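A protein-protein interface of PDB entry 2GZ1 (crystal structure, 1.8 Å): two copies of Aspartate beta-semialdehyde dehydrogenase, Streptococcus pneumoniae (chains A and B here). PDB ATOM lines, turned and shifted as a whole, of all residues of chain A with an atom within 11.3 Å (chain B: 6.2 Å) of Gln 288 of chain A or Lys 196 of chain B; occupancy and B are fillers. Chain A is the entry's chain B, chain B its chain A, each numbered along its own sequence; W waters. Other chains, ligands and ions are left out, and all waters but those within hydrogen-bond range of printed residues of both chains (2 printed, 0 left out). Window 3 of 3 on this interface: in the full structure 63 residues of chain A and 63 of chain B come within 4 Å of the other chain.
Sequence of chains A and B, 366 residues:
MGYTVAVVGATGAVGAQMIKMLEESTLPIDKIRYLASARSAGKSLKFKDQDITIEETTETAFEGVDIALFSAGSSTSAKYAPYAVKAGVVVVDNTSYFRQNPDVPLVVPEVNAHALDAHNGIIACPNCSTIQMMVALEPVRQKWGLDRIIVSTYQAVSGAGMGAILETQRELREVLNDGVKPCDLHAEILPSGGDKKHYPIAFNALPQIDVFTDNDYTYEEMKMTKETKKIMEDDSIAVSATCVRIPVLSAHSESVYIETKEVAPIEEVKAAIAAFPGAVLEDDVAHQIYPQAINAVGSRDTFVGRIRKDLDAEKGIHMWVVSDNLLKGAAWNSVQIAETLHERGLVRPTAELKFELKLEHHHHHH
The side-chain carboxylate (OD1) of Asp 195 of chain B lies close to the side-chain amide oxygen (OE1) of Gln 288 of chain A, at 3.4 Å.
The backbone carbonyl oxygen of His 287 of chain A sits close to the side-chain amino group of Lys 197 of chain B, 3.2 Å away.
The side-chain amide nitrogen (NE2) of Gln 288 of chain A is in hydrogen-bond range of the side-chain amide oxygen (OE1) of Gln 208 of chain B (3.0 Å).
The side-chain amide oxygen (OE1) of Gln 208 of chain B is in hydrogen-bond range of the side-chain hydroxyl (OH) of Tyr 290 of chain A (2.7 Å).
OH of Tyr 199 of chain B sits at hydrogen-bond distance from O of Gln 288 of chain A (2.7 Å).
The backbone NH (N) of Lys 197 of chain B is in hydrogen-bond range of the side-chain amide oxygen (OE1) of Gln 288 of chain A.
NE2 of Gln 208 of chain B sits at hydrogen-bond distance from OD2 of Asp 195 of chain B (3.0 Å).
The backbone carbonyl oxygen (O) of Asp 284 of chain A sits at hydrogen-bond distance from the backbone NH (N) of Ile 289 of chain A (3.0 Å).
The backbone NH of Arg 306 of chain A lies within hydrogen-bond range of the side-chain carboxylate of Asp 283 of chain A, at 3.5 Å.
The side-chain hydroxyl of Tyr 199 of chain B lies close to the side-chain amino group of Lys 197 of chain B (3.4 Å).
CG1 of Val 285 of chain A touches CE1 of Phe 212 of chain B (3.5 Å).
His 287 of chain A touches Tyr 199 of chain B (O to OH, 3.7 Å).
NE2 of Gln 288 of chain A touches CG of Pro 191 of chain B, at 3.8 Å.
Gln 288 of chain A touches Lys 196 of chain B (OE1 to N, 3.5 Å).
Ile 289 of chain A touches Lys 197 of chain B.
OH of Tyr 290 of chain A touches CG of Pro 191 of chain B, 3.4 Å away.
CE2 of Tyr 199 of chain B touches OH of Tyr 290 of chain A, at 3.4 Å.
NE2 of Gln 292 of chain A touches CD2 of Tyr 199 of chain B, at 3.4 Å.
Arg 306 of chain A touches Phe 212 of chain B (NE to CE1, 3.5 Å).
Printed residues of chain B within 4 Å of Val 285 of chain A: Phe 212.
Of chain B, only Pro 191, Asp 195, Lys 196, Lys 197, Tyr 199 and Gln 208 come within 4 Å of Gln 288 of chain A.
Of the printed residues of chain B, Ile 289 of chain A touches Lys 197 (3.7 Å).
Asn 295 of chain A touches none of the printed residues of chain B.
Pro 191 of chain B touches just these residues of chain A: Gln 288 and Tyr 290.
No residue of chain A comes within 4 Å of Ser 192 of chain B.
No residue of chain A comes within 4 Å of Gly 194 of chain B.
Asp 195 of chain B touches just one residue of chain A: Gln 288.
Lys 196 of chain B touches just one residue of chain A: Gln 288.
The nearest printed residue of chain A that does not touch Gln 208 of chain B is Arg 306 of chain A (5.0 Å).
Hydrophobic or aromatic side chains of chain B that line the printed part of chain A: Pro 191, Tyr 199 and Phe 212.
Among the printed residues, 15 pairs touch across the chains.
No position is printed for both chains.
Of the 15 pairs that touch across the chains among the printed residues, none has its exchanged pair printed and touching as well.
Water W1 lies within hydrogen-bond range of O of Lys 197 of chain B, O of Ser 192 of chain B and NE2 of Gln 288 of chain A.
Water W2 lies within hydrogen-bond range of OD1 of Asp 195 of chain B and O of Ala 286 of chain A.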
ATOM      1  N   LEU A 281      -8.719  10.397  15.795  1.00  0.00           N
ATOM      2  CA  LEU A 281      -8.341   9.000  15.921  1.00  0.00           C
ATOM      3  C   LEU A 281      -9.139   8.184  14.917  1.00  0.00           C
ATOM      4  O   LEU A 281     -10.355   8.170  14.968  1.00  0.00           O
ATOM      5  CB  LEU A 281      -8.624   8.502  17.338  1.00  0.00           C
ATOM      6  CG  LEU A 281      -8.156   7.085  17.673  1.00  0.00           C
ATOM      7  CD1 LEU A 281      -6.646   7.033  17.723  1.00  0.00           C
ATOM      8  CD2 LEU A 281      -8.752   6.661  18.993  1.00  0.00           C
ATOM      9  N   GLU A 282      -8.444   7.538  13.985  1.00  0.00           N
ATOM     10  CA  GLU A 282      -9.047   6.532  13.112  1.00  0.00           C
ATOM     11  C   GLU A 282      -8.304   5.241  13.388  1.00  0.00           C
ATOM     12  O   GLU A 282      -7.293   4.939  12.754  1.00  0.00           O
ATOM     13  CB  GLU A 282      -8.932   6.947  11.645  1.00  0.00           C
ATOM     14  CG  GLU A 282     -10.020   7.916  11.219  1.00  0.00           C
ATOM     15  CD  GLU A 282      -9.937   8.336   9.763  1.00  0.00           C
ATOM     16  OE1 GLU A 282      -8.883   8.118   9.115  1.00  0.00           O
ATOM     17  OE2 GLU A 282     -10.936   8.908   9.273  1.00  0.00           O
ATOM     18  N   ASP A 283      -8.782   4.496  14.373  1.00  0.00           N
ATOM     19  CA  ASP A 283      -8.036   3.339  14.854  1.00  0.00           C
ATOM     20  C   ASP A 283      -8.962   2.288  15.438  1.00  0.00           C
ATOM     21  O   ASP A 283      -9.323   2.340  16.608  1.00  0.00           O
ATOM     22  CB  ASP A 283      -7.006   3.792  15.872  1.00  0.00           C
ATOM     23  CG  ASP A 283      -5.894   2.763  16.094  1.00  0.00           C
ATOM     24  OD1 ASP A 283      -4.825   3.180  16.599  1.00  0.00           O
ATOM     25  OD2 ASP A 283      -6.009   1.540  15.800  1.00  0.00           O
ATOM     26  N   ASP A 284      -9.357   1.345  14.597  1.00  0.00           N
ATOM     27  CA  ASP A 284     -10.197   0.235  15.016  1.00  0.00           C
ATOM     28  C   ASP A 284      -9.854  -0.937  14.106  1.00  0.00           C
ATOM     29  O   ASP A 284     -10.512  -1.154  13.095  1.00  0.00           O
ATOM     30  CB  ASP A 284     -11.673   0.628  14.916  1.00  0.00           C
ATOM     31  CG  ASP A 284     -12.601  -0.478  15.337  1.00  0.00           C
ATOM     32  OD1 ASP A 284     -13.829  -0.264  15.292  1.00  0.00           O
ATOM     33  OD2 ASP A 284     -12.197  -1.597  15.719  1.00  0.00           O
ATOM     34  N   VAL A 285      -8.808  -1.680  14.466  1.00  0.00           N
ATOM     35  CA  VAL A 285      -8.276  -2.720  13.585  1.00  0.00           C
ATOM     36  C   VAL A 285      -9.228  -3.895  13.399  1.00  0.00           C
ATOM     37  O   VAL A 285      -9.146  -4.573  12.392  1.00  0.00           O
ATOM     38  CB  VAL A 285      -6.863  -3.219  14.026  1.00  0.00           C
ATOM     39  CG1 VAL A 285      -5.857  -2.078  13.950  1.00  0.00           C
ATOM     40  CG2 VAL A 285      -6.888  -3.839  15.411  1.00  0.00           C
ATOM     41  N   ALA A 286     -10.155  -4.099  14.336  1.00  0.00           N
ATOM     42  CA  ALA A 286     -11.184  -5.144  14.210  1.00  0.00           C
ATOM     43  C   ALA A 286     -12.077  -4.909  13.000  1.00  0.00           C
ATOM     44  O   ALA A 286     -12.682  -5.838  12.484  1.00  0.00           O
ATOM     45  CB  ALA A 286     -12.040  -5.214  15.476  1.00  0.00           C
ATOM     46  N   HIS A 287     -12.183  -3.654  12.569  1.00  0.00           N
ATOM     47  CA  HIS A 287     -12.948  -3.317  11.376  1.00  0.00           C
ATOM     48  C   HIS A 287     -12.078  -2.631  10.325  1.00  0.00           C
ATOM     49  O   HIS A 287     -12.580  -1.890   9.485  1.00  0.00           O
ATOM     50  CB  HIS A 287     -14.137  -2.444  11.763  1.00  0.00           C
ATOM     51  CG  HIS A 287     -15.069  -3.099  12.739  1.00  0.00           C
ATOM     52  ND1 HIS A 287     -15.903  -4.141  12.388  1.00  0.00           N
ATOM     53  CD2 HIS A 287     -15.290  -2.869  14.054  1.00  0.00           C
ATOM     54  CE1 HIS A 287     -16.607  -4.515  13.442  1.00  0.00           C
ATOM     55  NE2 HIS A 287     -16.249  -3.764  14.468  1.00  0.00           N
ATOM     56  N   GLN A 288     -10.776  -2.909  10.368  1.00  0.00           N
ATOM     57  CA  GLN A 288      -9.806  -2.381   9.408  1.00  0.00           C
ATOM     58  C   GLN A 288      -9.901  -0.862   9.223  1.00  0.00           C
ATOM     59  O   GLN A 288      -9.883  -0.350   8.092  1.00  0.00           O
ATOM     60  CB  GLN A 288      -9.967  -3.068   8.056  1.00  0.00           C
ATOM     61  CG  GLN A 288      -9.719  -4.567   8.066  1.00  0.00           C
ATOM     62  CD  GLN A 288     -10.184  -5.195   6.777  1.00  0.00           C
ATOM     63  OE1 GLN A 288     -11.295  -5.741   6.708  1.00  0.00           O
ATOM     64  NE2 GLN A 288      -9.364  -5.087   5.739  1.00  0.00           N
ATOM     65  N   ILE A 289      -9.992  -0.152  10.343  1.00  0.00           N
ATOM     66  CA  ILE A 289     -10.037   1.296  10.327  1.00  0.00           C
ATOM     67  C   ILE A 289      -8.658   1.845  10.673  1.00  0.00           C
ATOM     68  O   ILE A 289      -8.114   1.569  11.737  1.00  0.00           O
ATOM     69  CB  ILE A 289     -11.075   1.847  11.328  1.00  0.00           C
ATOM     70  CG1 ILE A 289     -12.472   1.282  11.063  1.00  0.00           C
ATOM     71  CG2 ILE A 289     -11.082   3.393  11.294  1.00  0.00           C
ATOM     72  CD1 ILE A 289     -13.107   1.734   9.778  1.00  0.00           C
ATOM     73  N   TYR A 290      -8.125   2.635   9.753  1.00  0.00           N
ATOM     74  CA  TYR A 290      -6.865   3.319   9.920  1.00  0.00           C
ATOM     75  C   TYR A 290      -6.864   4.506   8.951  1.00  0.00           C
ATOM     76  O   TYR A 290      -7.636   4.537   7.989  1.00  0.00           O
ATOM     77  CB  TYR A 290      -5.686   2.370   9.642  1.00  0.00           C
ATOM     78  CG  TYR A 290      -5.966   1.321   8.584  1.00  0.00           C
ATOM     79  CD1 TYR A 290      -6.145   1.671   7.246  1.00  0.00           C
ATOM     80  CD2 TYR A 290      -6.103  -0.019   8.928  1.00  0.00           C
ATOM     81  CE1 TYR A 290      -6.403   0.707   6.275  1.00  0.00           C
ATOM     82  CE2 TYR A 290      -6.365  -0.983   7.975  1.00  0.00           C
ATOM     83  CZ  TYR A 290      -6.526  -0.621   6.648  1.00  0.00           C
ATOM     84  OH  TYR A 290      -6.782  -1.600   5.706  1.00  0.00           O
ATOM     85  N   PRO A 291      -6.026   5.505   9.199  1.00  0.00           N
ATOM     86  CA  PRO A 291      -5.945   6.636   8.277  1.00  0.00           C
ATOM     87  C   PRO A 291      -5.536   6.196   6.873  1.00  0.00           C
ATOM     88  O   PRO A 291      -4.722   5.289   6.731  1.00  0.00           O
ATOM     89  CB  PRO A 291      -4.880   7.539   8.907  1.00  0.00           C
ATOM     90  CG  PRO A 291      -4.845   7.150  10.372  1.00  0.00           C
ATOM     91  CD  PRO A 291      -5.138   5.664  10.365  1.00  0.00           C
ATOM     92  N   GLN A 292      -6.129   6.817   5.861  1.00  0.00           N
ATOM     93  CA  GLN A 292      -5.772   6.582   4.466  1.00  0.00           C
ATOM     94  C   GLN A 292      -5.686   7.917   3.738  1.00  0.00           C
ATOM     95  O   GLN A 292      -6.612   8.741   3.837  1.00  0.00           O
ATOM     96  CB  GLN A 292      -6.843   5.741   3.773  1.00  0.00           C
ATOM     97  CG  GLN A 292      -7.067   4.370   4.373  1.00  0.00           C
ATOM     98  CD  GLN A 292      -8.094   3.539   3.602  1.00  0.00           C
ATOM     99  OE1 GLN A 292      -8.207   3.654   2.376  1.00  0.00           O
ATOM    100  NE2 GLN A 292      -8.831   2.685   4.319  1.00  0.00           N
ATOM    101  N   ALA A 293      -4.621   8.105   2.965  1.00  0.00           N
ATOM    102  CA  ALA A 293      -4.461   9.296   2.114  1.00  0.00           C
ATOM    103  C   ALA A 293      -5.752   9.671   1.385  1.00  0.00           C
ATOM    104  O   ALA A 293      -6.182  10.820   1.432  1.00  0.00           O
ATOM    105  CB  ALA A 293      -3.353   9.069   1.105  1.00  0.00           C
ATOM    106  N   ILE A 294      -6.390   8.707   0.725  1.00  0.00           N
ATOM    107  CA  ILE A 294      -7.557   9.027  -0.089  1.00  0.00           C
ATOM    108  C   ILE A 294      -8.736   9.531   0.765  1.00  0.00           C
ATOM    109  O   ILE A 294      -9.571  10.285   0.273  1.00  0.00           O
ATOM    110  CB  ILE A 294      -7.990   7.863  -1.038  1.00  0.00           C
ATOM    111  CG1 ILE A 294      -8.469   6.624  -0.253  1.00  0.00           C
ATOM    112  CG2 ILE A 294      -6.858   7.507  -1.990  1.00  0.00           C
ATOM    113  CD1 ILE A 294      -8.935   5.484  -1.131  1.00  0.00           C
ATOM    114  N   ASN A 295      -8.794   9.129   2.029  1.00  0.00           N
ATOM    115  CA  ASN A 295      -9.847   9.613   2.927  1.00  0.00           C
ATOM    116  C   ASN A 295      -9.559  10.986   3.534  1.00  0.00           C
ATOM    117  O   ASN A 295     -10.492  11.746   3.828  1.00  0.00           O
ATOM    118  CB  ASN A 295     -10.145   8.581   4.021  1.00  0.00           C
ATOM    119  CG  ASN A 295     -10.837   7.341   3.481  1.00  0.00           C
ATOM    120  OD1 ASN A 295     -11.477   7.372   2.423  1.00  0.00           O
ATOM    121  ND2 ASN A 295     -10.706   6.243   4.198  1.00  0.00           N
ATOM    122  N   VAL A 304      -4.894   9.757  12.768  1.00  0.00           N
ATOM    123  CA  VAL A 304      -3.895   8.926  13.432  1.00  0.00           C
ATOM    124  C   VAL A 304      -4.460   7.567  13.776  1.00  0.00           C
ATOM    125  O   VAL A 304      -5.563   7.457  14.333  1.00  0.00           O
ATOM    126  CB  VAL A 304      -3.371   9.594  14.719  1.00  0.00           C
ATOM    127  CG1 VAL A 304      -2.176   8.823  15.281  1.00  0.00           C
ATOM    128  CG2 VAL A 304      -2.991  11.035  14.464  1.00  0.00           C
ATOM    129  N   GLY A 305      -3.709   6.524  13.427  1.00  0.00           N
ATOM    130  CA  GLY A 305      -4.067   5.160  13.786  1.00  0.00           C
ATOM    131  C   GLY A 305      -2.862   4.235  13.771  1.00  0.00           C
ATOM    132  O   GLY A 305      -1.713   4.681  13.872  1.00  0.00           O
ATOM    133  N   ARG A 306      -3.144   2.948  13.595  1.00  0.00           N
ATOM    134  CA  ARG A 306      -2.186   1.856  13.773  1.00  0.00           C
ATOM    135  C   ARG A 306      -1.364   2.022  15.055  1.00  0.00           C
ATOM    136  O   ARG A 306      -0.203   1.636  15.109  1.00  0.00           O
ATOM    137  CB  ARG A 306      -1.261   1.716  12.556  1.00  0.00           C
ATOM    138  CG  ARG A 306      -1.931   1.317  11.224  1.00  0.00           C
ATOM    139  CD  ARG A 306      -2.638  -0.053  11.218  1.00  0.00           C
ATOM    140  NE  ARG A 306      -1.915  -1.050  12.008  1.00  0.00           N
ATOM    141  CZ  ARG A 306      -0.808  -1.674  11.631  1.00  0.00           C
ATOM    142  NH1 ARG A 306      -0.274  -1.480  10.434  1.00  0.00           N
ATOM    143  NH2 ARG A 306      -0.249  -2.541  12.456  1.00  0.00           N
ATOM    144  N   ILE A 307      -1.973   2.579  16.088  1.00  0.00           N
ATOM    145  CA  ILE A 307      -1.248   2.911  17.297  1.00  0.00           C
ATOM    146  C   ILE A 307      -1.016   1.626  18.077  1.00  0.00           C
ATOM    147  O   ILE A 307      -1.955   0.872  18.359  1.00  0.00           O
ATOM    148  CB  ILE A 307      -1.991   3.943  18.166  1.00  0.00           C
ATOM    149  CG1 ILE A 307      -2.178   5.269  17.417  1.00  0.00           C
ATOM    150  CG2 ILE A 307      -1.198   4.195  19.438  1.00  0.00           C
ATOM    151  CD1 ILE A 307      -3.288   6.133  17.993  1.00  0.00           C
ATOM    152  N   TRP A 320       0.576   5.605  12.568  1.00  0.00           N
ATOM    153  CA  TRP A 320       0.400   5.968  11.162  1.00  0.00           C
ATOM    154  C   TRP A 320      -0.357   7.290  11.173  1.00  0.00           C
ATOM    155  O   TRP A 320      -1.441   7.382  11.739  1.00  0.00           O
ATOM    156  CB  TRP A 320      -0.411   4.878  10.474  1.00  0.00           C
ATOM    157  CG  TRP A 320      -0.663   5.020   8.986  1.00  0.00           C
ATOM    158  CD1 TRP A 320      -1.865   5.218   8.366  1.00  0.00           C
ATOM    159  CD2 TRP A 320       0.304   4.916   7.950  1.00  0.00           C
ATOM    160  NE1 TRP A 320      -1.702   5.243   7.003  1.00  0.00           N
ATOM    161  CE2 TRP A 320      -0.378   5.067   6.716  1.00  0.00           C
ATOM    162  CE3 TRP A 320       1.689   4.706   7.927  1.00  0.00           C
ATOM    163  CZ2 TRP A 320       0.270   5.020   5.492  1.00  0.00           C
ATOM    164  CZ3 TRP A 320       2.330   4.664   6.705  1.00  0.00           C
ATOM    165  CH2 TRP A 320       1.615   4.824   5.499  1.00  0.00           C
ATOM    166  N   PRO B 191      -6.966  -4.320   0.903  1.00  0.00           N
ATOM    167  CA  PRO B 191      -5.587  -4.711   1.245  1.00  0.00           C
ATOM    168  C   PRO B 191      -5.292  -6.217   1.386  1.00  0.00           C
ATOM    169  O   PRO B 191      -4.132  -6.617   1.264  1.00  0.00           O
ATOM    170  CB  PRO B 191      -5.383  -4.036   2.609  1.00  0.00           C
ATOM    171  CG  PRO B 191      -6.738  -3.952   3.188  1.00  0.00           C
ATOM    172  CD  PRO B 191      -7.642  -3.671   2.041  1.00  0.00           C
ATOM    173  N   SER B 192      -6.308  -7.017   1.667  1.00  0.00           N
ATOM    174  CA  SER B 192      -6.145  -8.456   1.870  1.00  0.00           C
ATOM    175  C   SER B 192      -7.387  -9.203   1.400  1.00  0.00           C
ATOM    176  O   SER B 192      -8.493  -8.950   1.873  1.00  0.00           O
ATOM    177  CB  SER B 192      -5.879  -8.760   3.346  1.00  0.00           C
ATOM    178  OG  SER B 192      -5.931 -10.154   3.595  1.00  0.00           O
ATOM    179  N   GLY B 193      -7.185 -10.126   0.463  1.00  0.00           N
ATOM    180  CA  GLY B 193      -8.265 -10.851  -0.178  1.00  0.00           C
ATOM    181  C   GLY B 193      -9.167 -11.586   0.792  1.00  0.00           C
ATOM    182  O   GLY B 193     -10.369 -11.650   0.575  1.00  0.00           O
ATOM    183  N   GLY B 194      -8.593 -12.133   1.862  1.00  0.00           N
ATOM    184  CA  GLY B 194      -9.358 -12.919   2.817  1.00  0.00           C
ATOM    185  C   GLY B 194     -10.150 -12.095   3.822  1.00  0.00           C
ATOM    186  O   GLY B 194     -11.113 -12.595   4.402  1.00  0.00           O
ATOM    187  N   ASP B 195      -9.763 -10.839   4.024  1.00  0.00           N
ATOM    188  CA  ASP B 195     -10.392  -9.996   5.050  1.00  0.00           C
ATOM    189  C   ASP B 195     -11.764  -9.467   4.602  1.00  0.00           C
ATOM    190  O   ASP B 195     -12.165  -9.617   3.441  1.00  0.00           O
ATOM    191  CB  ASP B 195      -9.465  -8.835   5.459  1.00  0.00           C
ATOM    192  CG  ASP B 195      -9.484  -8.556   6.970  1.00  0.00           C
ATOM    193  OD1 ASP B 195     -10.449  -8.929   7.678  1.00  0.00           O
ATOM    194  OD2 ASP B 195      -8.570  -7.953   7.542  1.00  0.00           O
ATOM    195  N   LYS B 196     -12.469  -8.855   5.548  1.00  0.00           N
ATOM    196  CA  LYS B 196     -13.875  -8.494   5.391  1.00  0.00           C
ATOM    197  C   LYS B 196     -14.084  -7.311   4.466  1.00  0.00           C
ATOM    198  O   LYS B 196     -15.008  -7.311   3.660  1.00  0.00           O
ATOM    199  CB  LYS B 196     -14.473  -8.144   6.754  1.00  0.00           C
ATOM    200  CG  LYS B 196     -14.547  -9.302   7.741  1.00  0.00           C
ATOM    201  CD  LYS B 196     -15.185  -8.858   9.053  1.00  0.00           C
ATOM    202  CE  LYS B 196     -15.580 -10.049   9.915  1.00  0.00           C
ATOM    203  NZ  LYS B 196     -14.403 -10.900  10.244  1.00  0.00           N
ATOM    204  N   LYS B 197     -13.227  -6.301   4.596  1.00  0.00           N
ATOM    205  CA  LYS B 197     -13.392  -5.049   3.877  1.00  0.00           C
ATOM    206  C   LYS B 197     -12.253  -4.823   2.905  1.00  0.00           C
ATOM    207  O   LYS B 197     -11.102  -5.152   3.190  1.00  0.00           O
ATOM    208  CB  LYS B 197     -13.465  -3.878   4.863  1.00  0.00           C
ATOM    209  CG  LYS B 197     -14.650  -3.983   5.817  1.00  0.00           C
ATOM    210  CD  LYS B 197     -15.221  -2.629   6.177  1.00  0.00           C
ATOM    211  CE  LYS B 197     -14.544  -2.090   7.386  1.00  0.00           C
ATOM    212  NZ  LYS B 197     -14.866  -0.694   7.671  1.00  0.00           N
ATOM    213  N   HIS B 198     -12.586  -4.226   1.769  1.00  0.00           N
ATOM    214  CA  HIS B 198     -11.609  -3.908   0.741  1.00  0.00           C
ATOM    215  C   HIS B 198     -11.588  -2.411   0.438  1.00  0.00           C
ATOM    216  O   HIS B 198     -12.614  -1.744   0.481  1.00  0.00           O
ATOM    217  CB  HIS B 198     -11.918  -4.721  -0.501  1.00  0.00           C
ATOM    218  CG  HIS B 198     -12.058  -6.180  -0.220  1.00  0.00           C
ATOM    219  ND1 HIS B 198     -10.970  -7.010  -0.065  1.00  0.00           N
ATOM    220  CD2 HIS B 198     -13.150  -6.944   0.006  1.00  0.00           C
ATOM    221  CE1 HIS B 198     -11.391  -8.236   0.195  1.00  0.00           C
ATOM    222  NE2 HIS B 198     -12.709  -8.220   0.247  1.00  0.00           N
ATOM    223  N   TYR B 199     -10.400  -1.900   0.157  1.00  0.00           N
ATOM    224  CA  TYR B 199     -10.169  -0.476  -0.049  1.00  0.00           C
ATOM    225  C   TYR B 199      -9.379  -0.218  -1.330  1.00  0.00           C
ATOM    226  O   TYR B 199      -8.538  -1.035  -1.719  1.00  0.00           O
ATOM    227  CB  TYR B 199      -9.365   0.083   1.123  1.00  0.00           C
ATOM    228  CG  TYR B 199     -10.024  -0.072   2.471  1.00  0.00           C
ATOM    229  CD1 TYR B 199     -11.341   0.321   2.673  1.00  0.00           C
ATOM    230  CD2 TYR B 199      -9.317  -0.585   3.552  1.00  0.00           C
ATOM    231  CE1 TYR B 199     -11.954   0.180   3.903  1.00  0.00           C
ATOM    232  CE2 TYR B 199      -9.908  -0.712   4.794  1.00  0.00           C
ATOM    233  CZ  TYR B 199     -11.229  -0.330   4.963  1.00  0.00           C
ATOM    234  OH  TYR B 199     -11.819  -0.459   6.189  1.00  0.00           O
ATOM    235  N   GLN B 208      -1.975  -1.859   5.787  1.00  0.00           N
ATOM    236  CA  GLN B 208      -2.382  -3.211   6.128  1.00  0.00           C
ATOM    237  C   GLN B 208      -1.964  -4.144   5.034  1.00  0.00           C
ATOM    238  O   GLN B 208      -2.353  -3.990   3.877  1.00  0.00           O
ATOM    239  CB  GLN B 208      -3.879  -3.350   6.365  1.00  0.00           C
ATOM    240  CG  GLN B 208      -4.284  -4.821   6.627  1.00  0.00           C
ATOM    241  CD  GLN B 208      -5.772  -5.093   6.667  1.00  0.00           C
ATOM    242  OE1 GLN B 208      -6.602  -4.176   6.610  1.00  0.00           O
ATOM    243  NE2 GLN B 208      -6.124  -6.381   6.761  1.00  0.00           N
ATOM    244  N   PHE B 212      -5.052  -8.778  10.572  1.00  0.00           N
ATOM    245  CA  PHE B 212      -4.553  -8.376  11.893  1.00  0.00           C
ATOM    246  C   PHE B 212      -4.450  -9.540  12.853  1.00  0.00           C
ATOM    247  O   PHE B 212      -5.321 -10.406  12.870  1.00  0.00           O
ATOM    248  CB  PHE B 212      -5.436  -7.283  12.502  1.00  0.00           C
ATOM    249  CG  PHE B 212      -5.208  -5.942  11.876  1.00  0.00           C
ATOM    250  CD1 PHE B 212      -4.160  -5.138  12.300  1.00  0.00           C
ATOM    251  CD2 PHE B 212      -6.000  -5.517  10.824  1.00  0.00           C
ATOM    252  CE1 PHE B 212      -3.932  -3.908  11.705  1.00  0.00           C
ATOM    253  CE2 PHE B 212      -5.783  -4.295  10.225  1.00  0.00           C
ATOM    254  CZ  PHE B 212      -4.747  -3.487  10.655  1.00  0.00           C
HETATM  255  O   HOH W   1      -8.894  -6.469   2.744  1.00  0.00           O
HETATM  256  O   HOH W   2     -11.490  -7.807   9.995  1.00  0.00           O
